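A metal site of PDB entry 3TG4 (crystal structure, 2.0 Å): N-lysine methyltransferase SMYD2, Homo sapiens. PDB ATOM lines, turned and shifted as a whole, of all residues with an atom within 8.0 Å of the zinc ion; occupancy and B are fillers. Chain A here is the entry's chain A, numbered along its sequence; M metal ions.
The zinc ion is bound by a ring nitrogen (NE2) of His 86, the side-chain sulfur of Cys 68, the side-chain sulfur of Cys 90 and the side-chain sulfur of Cys 65.
Four residues have an atom within 4 Å of the zinc ion: Cys 65, Cys 68, His 86 and Cys 90. The nearest printed residue that does not touch the zinc ion is Arg 67 (4.4 Å).
The side-chain sulfur of Cys 68 lies close to the backbone NH of Gln 70. SG of Cys 65 lies close to N of Arg 67, 3.6 Å away. The backbone NH (N) of Cys 65 is in hydrogen-bond range of the backbone carbonyl oxygen (O) of Ala 71.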
ATOM      1  N   LYS A  64      -2.857  25.605 -19.891  1.00  0.00           N
ATOM      2  CA  LYS A  64      -2.480  26.717 -20.768  1.00  0.00           C
ATOM      3  C   LYS A  64      -0.989  26.701 -21.164  1.00  0.00           C
ATOM      4  O   LYS A  64      -0.143  26.509 -20.312  1.00  0.00           O
ATOM      5  CB  LYS A  64      -2.791  28.039 -20.038  1.00  0.00           C
ATOM      6  CG  LYS A  64      -2.664  29.312 -20.883  1.00  0.00           C
ATOM      7  CD  LYS A  64      -3.103  30.542 -20.093  1.00  0.00           C
ATOM      8  CE  LYS A  64      -2.123  30.880 -18.997  1.00  0.00           C
ATOM      9  NZ  LYS A  64      -2.779  31.623 -17.913  1.00  0.00           N
ATOM     10  N   CYS A  65      -0.674  26.942 -22.437  1.00  0.00           N
ATOM     11  CA  CYS A  65       0.723  27.178 -22.824  1.00  0.00           C
ATOM     12  C   CYS A  65       1.266  28.387 -22.051  1.00  0.00           C
ATOM     13  O   CYS A  65       0.688  29.456 -22.088  1.00  0.00           O
ATOM     14  CB  CYS A  65       0.876  27.416 -24.318  1.00  0.00           C
ATOM     15  SG  CYS A  65       2.582  27.780 -24.832  1.00  0.00           S
ATOM     16  N   GLY A  66       2.384  28.193 -21.359  1.00  0.00           N
ATOM     17  CA  GLY A  66       2.947  29.218 -20.491  1.00  0.00           C
ATOM     18  C   GLY A  66       3.678  30.347 -21.206  1.00  0.00           C
ATOM     19  O   GLY A  66       3.924  31.395 -20.609  1.00  0.00           O
ATOM     20  N   ARG A  67       4.042  30.127 -22.472  1.00  0.00           N
ATOM     21  CA  ARG A  67       4.751  31.143 -23.255  1.00  0.00           C
ATOM     22  C   ARG A  67       3.760  32.161 -23.851  1.00  0.00           C
ATOM     23  O   ARG A  67       3.890  33.357 -23.608  1.00  0.00           O
ATOM     24  CB  ARG A  67       5.558  30.531 -24.411  1.00  0.00           C
ATOM     25  CG  ARG A  67       6.586  29.455 -24.070  1.00  0.00           C
ATOM     26  CD  ARG A  67       7.226  28.933 -25.387  1.00  0.00           C
ATOM     27  NE  ARG A  67       8.182  27.848 -25.147  1.00  0.00           N
ATOM     28  CZ  ARG A  67       7.924  26.551 -25.290  1.00  0.00           C
ATOM     29  NH1 ARG A  67       6.719  26.145 -25.706  1.00  0.00           N
ATOM     30  NH2 ARG A  67       8.862  25.655 -25.028  1.00  0.00           N
ATOM     31  N   CYS A  68       2.791  31.671 -24.626  1.00  0.00           N
ATOM     32  CA  CYS A  68       1.876  32.576 -25.318  1.00  0.00           C
ATOM     33  C   CYS A  68       0.579  32.808 -24.551  1.00  0.00           C
ATOM     34  O   CYS A  68      -0.104  33.807 -24.787  1.00  0.00           O
ATOM     35  CB  CYS A  68       1.559  32.057 -26.704  1.00  0.00           C
ATOM     36  SG  CYS A  68       0.653  30.523 -26.681  1.00  0.00           S
ATOM     37  N   LYS A  69       0.242  31.870 -23.662  1.00  0.00           N
ATOM     38  CA  LYS A  69      -1.005  31.930 -22.874  1.00  0.00           C
ATOM     39  C   LYS A  69      -2.270  31.924 -23.739  1.00  0.00           C
ATOM     40  O   LYS A  69      -3.343  32.328 -23.294  1.00  0.00           O
ATOM     41  CB  LYS A  69      -0.974  33.129 -21.906  1.00  0.00           C
ATOM     42  CG  LYS A  69       0.299  33.193 -21.079  1.00  0.00           C
ATOM     43  CD  LYS A  69       0.346  34.432 -20.205  1.00  0.00           C
ATOM     44  CE  LYS A  69       1.770  34.697 -19.722  1.00  0.00           C
ATOM     45  NZ  LYS A  69       2.281  33.564 -18.912  1.00  0.00           N
ATOM     46  N   GLN A  70      -2.158  31.447 -24.972  1.00  0.00           N
ATOM     47  CA  GLN A  70      -3.265  31.462 -25.918  1.00  0.00           C
ATOM     48  C   GLN A  70      -3.423  30.129 -26.653  1.00  0.00           C
ATOM     49  O   GLN A  70      -3.949  30.066 -27.765  1.00  0.00           O
ATOM     50  CB  GLN A  70      -3.107  32.632 -26.904  1.00  0.00           C
ATOM     51  CG  GLN A  70      -3.360  33.993 -26.233  1.00  0.00           C
ATOM     52  CD  GLN A  70      -3.414  35.134 -27.223  1.00  0.00           C
ATOM     53  OE1 GLN A  70      -4.401  35.298 -27.938  1.00  0.00           O
ATOM     54  NE2 GLN A  70      -2.358  35.938 -27.273  1.00  0.00           N
ATOM     55  N   ALA A  71      -2.967  29.058 -26.013  1.00  0.00           N
ATOM     56  CA  ALA A  71      -3.207  27.703 -26.490  1.00  0.00           C
ATOM     57  C   ALA A  71      -3.441  26.836 -25.261  1.00  0.00           C
ATOM     58  O   ALA A  71      -2.722  26.998 -24.260  1.00  0.00           O
ATOM     59  CB  ALA A  71      -2.003  27.188 -27.297  1.00  0.00           C
ATOM     60  N   PHE A  72      -4.435  25.932 -25.339  1.00  0.00           N
ATOM     61  CA  PHE A  72      -4.844  25.090 -24.193  1.00  0.00           C
ATOM     62  C   PHE A  72      -4.938  23.607 -24.544  1.00  0.00           C
ATOM     63  O   PHE A  72      -5.305  23.243 -25.665  1.00  0.00           O
ATOM     64  CB  PHE A  72      -6.187  25.585 -23.617  1.00  0.00           C
ATOM     65  CG  PHE A  72      -6.159  27.018 -23.131  1.00  0.00           C
ATOM     66  CD1 PHE A  72      -6.095  27.303 -21.786  1.00  0.00           C
ATOM     67  CD2 PHE A  72      -6.204  28.079 -24.040  1.00  0.00           C
ATOM     68  CE1 PHE A  72      -6.098  28.619 -21.332  1.00  0.00           C
ATOM     69  CE2 PHE A  72      -6.196  29.405 -23.599  1.00  0.00           C
ATOM     70  CZ  PHE A  72      -6.135  29.676 -22.237  1.00  0.00           C
ATOM     71  N   TYR A  73      -4.593  22.753 -23.590  1.00  0.00           N
ATOM     72  CA  TYR A  73      -4.425  21.317 -23.832  1.00  0.00           C
ATOM     73  C   TYR A  73      -5.003  20.474 -22.706  1.00  0.00           C
ATOM     74  O   TYR A  73      -5.144  20.949 -21.580  1.00  0.00           O
ATOM     75  CB  TYR A  73      -2.938  20.981 -23.985  1.00  0.00           C
ATOM     76  CG  TYR A  73      -2.280  21.724 -25.113  1.00  0.00           C
ATOM     77  CD1 TYR A  73      -2.388  21.273 -26.433  1.00  0.00           C
ATOM     78  CD2 TYR A  73      -1.554  22.886 -24.870  1.00  0.00           C
ATOM     79  CE1 TYR A  73      -1.780  21.959 -27.463  1.00  0.00           C
ATOM     80  CE2 TYR A  73      -0.949  23.580 -25.911  1.00  0.00           C
ATOM     81  CZ  TYR A  73      -1.048  23.103 -27.199  1.00  0.00           C
ATOM     82  OH  TYR A  73      -0.451  23.786 -28.210  1.00  0.00           O
ATOM     83  N   GLN A  79      -0.089  18.775 -25.174  1.00  0.00           N
ATOM     84  CA  GLN A  79       0.758  19.953 -25.382  1.00  0.00           C
ATOM     85  C   GLN A  79       2.048  19.640 -26.176  1.00  0.00           C
ATOM     86  O   GLN A  79       2.424  20.380 -27.109  1.00  0.00           O
ATOM     87  CB  GLN A  79       1.096  20.654 -24.056  1.00  0.00           C
ATOM     88  CG  GLN A  79       1.929  21.929 -24.256  1.00  0.00           C
ATOM     89  CD  GLN A  79       2.233  22.674 -22.969  1.00  0.00           C
ATOM     90  OE1 GLN A  79       2.831  23.760 -22.998  1.00  0.00           O
ATOM     91  NE2 GLN A  79       1.861  22.099 -21.844  1.00  0.00           N
ATOM     92  N   ASP A  82       1.293  18.651 -29.899  1.00  0.00           N
ATOM     93  CA  ASP A  82       0.859  19.790 -30.714  1.00  0.00           C
ATOM     94  C   ASP A  82       2.001  20.744 -31.064  1.00  0.00           C
ATOM     95  O   ASP A  82       1.855  21.586 -31.950  1.00  0.00           O
ATOM     96  CB  ASP A  82      -0.252  20.565 -29.997  1.00  0.00           C
ATOM     97  CG  ASP A  82      -1.002  21.496 -30.918  1.00  0.00           C
ATOM     98  OD1 ASP A  82      -1.461  21.025 -31.992  1.00  0.00           O
ATOM     99  OD2 ASP A  82      -1.143  22.708 -30.578  1.00  0.00           O
ATOM    100  N   TRP A  83       3.132  20.606 -30.376  1.00  0.00           N
ATOM    101  CA  TRP A  83       4.213  21.591 -30.469  1.00  0.00           C
ATOM    102  C   TRP A  83       4.770  21.842 -31.902  1.00  0.00           C
ATOM    103  O   TRP A  83       4.987  23.000 -32.248  1.00  0.00           O
ATOM    104  CB  TRP A  83       5.328  21.290 -29.462  1.00  0.00           C
ATOM    105  CG  TRP A  83       6.510  22.219 -29.563  1.00  0.00           C
ATOM    106  CD1 TRP A  83       7.797  21.865 -29.874  1.00  0.00           C
ATOM    107  CD2 TRP A  83       6.520  23.645 -29.349  1.00  0.00           C
ATOM    108  NE1 TRP A  83       8.601  22.990 -29.879  1.00  0.00           N
ATOM    109  CE2 TRP A  83       7.839  24.086 -29.563  1.00  0.00           C
ATOM    110  CE3 TRP A  83       5.534  24.578 -29.004  1.00  0.00           C
ATOM    111  CZ2 TRP A  83       8.218  25.441 -29.423  1.00  0.00           C
ATOM    112  CZ3 TRP A  83       5.897  25.933 -28.879  1.00  0.00           C
ATOM    113  CH2 TRP A  83       7.235  26.343 -29.086  1.00  0.00           C
ATOM    114  N   HIS A  86       2.091  24.105 -33.142  1.00  0.00           N
ATOM    115  CA  HIS A  86       1.836  25.260 -32.303  1.00  0.00           C
ATOM    116  C   HIS A  86       2.973  26.298 -32.349  1.00  0.00           C
ATOM    117  O   HIS A  86       2.734  27.504 -32.193  1.00  0.00           O
ATOM    118  CB  HIS A  86       1.586  24.854 -30.846  1.00  0.00           C
ATOM    119  CG  HIS A  86       1.397  26.021 -29.940  1.00  0.00           C
ATOM    120  ND1 HIS A  86       0.462  26.999 -30.191  1.00  0.00           N
ATOM    121  CD2 HIS A  86       2.049  26.399 -28.826  1.00  0.00           C
ATOM    122  CE1 HIS A  86       0.549  27.932 -29.262  1.00  0.00           C
ATOM    123  NE2 HIS A  86       1.483  27.583 -28.406  1.00  0.00           N
ATOM    124  N   LYS A  87       4.200  25.823 -32.547  1.00  0.00           N
ATOM    125  CA  LYS A  87       5.372  26.695 -32.627  1.00  0.00           C
ATOM    126  C   LYS A  87       5.336  27.692 -33.789  1.00  0.00           C
ATOM    127  O   LYS A  87       6.012  28.716 -33.740  1.00  0.00           O
ATOM    128  CB  LYS A  87       6.667  25.864 -32.679  1.00  0.00           C
ATOM    129  CG  LYS A  87       6.835  25.067 -33.949  1.00  0.00           C
ATOM    130  CD  LYS A  87       7.832  23.927 -33.736  1.00  0.00           C
ATOM    131  CE  LYS A  87       9.263  24.383 -33.856  1.00  0.00           C
ATOM    132  NZ  LYS A  87      10.179  23.201 -33.751  1.00  0.00           N
ATOM    133  N   GLU A  89       2.941  29.561 -34.268  1.00  0.00           N
ATOM    134  CA  GLU A  89       2.129  30.690 -33.760  1.00  0.00           C
ATOM    135  C   GLU A  89       2.466  31.147 -32.346  1.00  0.00           C
ATOM    136  O   GLU A  89       2.107  32.263 -31.962  1.00  0.00           O
ATOM    137  CB  GLU A  89       0.631  30.346 -33.840  1.00  0.00           C
ATOM    138  CG  GLU A  89       0.153  30.129 -35.280  1.00  0.00           C
ATOM    139  CD  GLU A  89      -1.309  29.656 -35.391  1.00  0.00           C
ATOM    140  OE1 GLU A  89      -1.824  29.071 -34.415  1.00  0.00           O
ATOM    141  OE2 GLU A  89      -1.908  29.865 -36.473  1.00  0.00           O
ATOM    142  N   CYS A  90       3.146  30.298 -31.573  1.00  0.00           N
ATOM    143  CA  CYS A  90       3.390  30.564 -30.152  1.00  0.00           C
ATOM    144  C   CYS A  90       4.183  31.859 -29.957  1.00  0.00           C
ATOM    145  O   CYS A  90       3.685  32.801 -29.323  1.00  0.00           O
ATOM    146  CB  CYS A  90       4.134  29.385 -29.481  1.00  0.00           C
ATOM    147  SG  CYS A  90       4.317  29.581 -27.652  1.00  0.00           S
ATOM    148  N   SER A  91       5.389  31.914 -30.508  1.00  0.00           N
ATOM    149  CA  SER A  91       6.182  33.142 -30.435  1.00  0.00           C
ATOM    150  C   SER A  91       5.561  34.333 -31.194  1.00  0.00           C
ATOM    151  O   SER A  91       5.564  35.455 -30.649  1.00  0.00           O
ATOM    152  CB  SER A  91       7.634  32.906 -30.833  1.00  0.00           C
ATOM    153  OG  SER A  91       8.394  34.078 -30.648  1.00  0.00           O
ATOM    154  N   MET A  93       2.466  35.103 -31.664  1.00  0.00           N
ATOM    155  CA  MET A  93       1.392  35.672 -30.856  1.00  0.00           C
ATOM    156  C   MET A  93       1.921  36.580 -29.739  1.00  0.00           C
ATOM    157  O   MET A  93       1.291  37.584 -29.403  1.00  0.00           O
ATOM    158  CB  MET A  93       0.495  34.580 -30.301  1.00  0.00           C
ATOM    159  CG  MET A  93      -0.456  34.009 -31.335  1.00  0.00           C
ATOM    160  SD  MET A  93      -1.675  32.930 -30.542  1.00  0.00           S
ATOM    161  CE  MET A  93      -0.707  31.458 -30.231  1.00  0.00           C
ATOM    162  N   VAL A  94       3.086  36.239 -29.182  1.00  0.00           N
ATOM    163  CA  VAL A  94       3.720  37.113 -28.177  1.00  0.00           C
ATOM    164  C   VAL A  94       4.278  38.372 -28.850  1.00  0.00           C
ATOM    165  O   VAL A  94       4.104  39.505 -28.370  1.00  0.00           O
ATOM    166  CB  VAL A  94       4.852  36.395 -27.388  1.00  0.00           C
ATOM    167  CG1 VAL A  94       5.553  37.372 -26.410  1.00  0.00           C
ATOM    168  CG2 VAL A  94       4.300  35.171 -26.632  1.00  0.00           C
HETATM  169 ZN    ZN M   1       2.244  28.882 -26.876  1.00  0.00          ZN
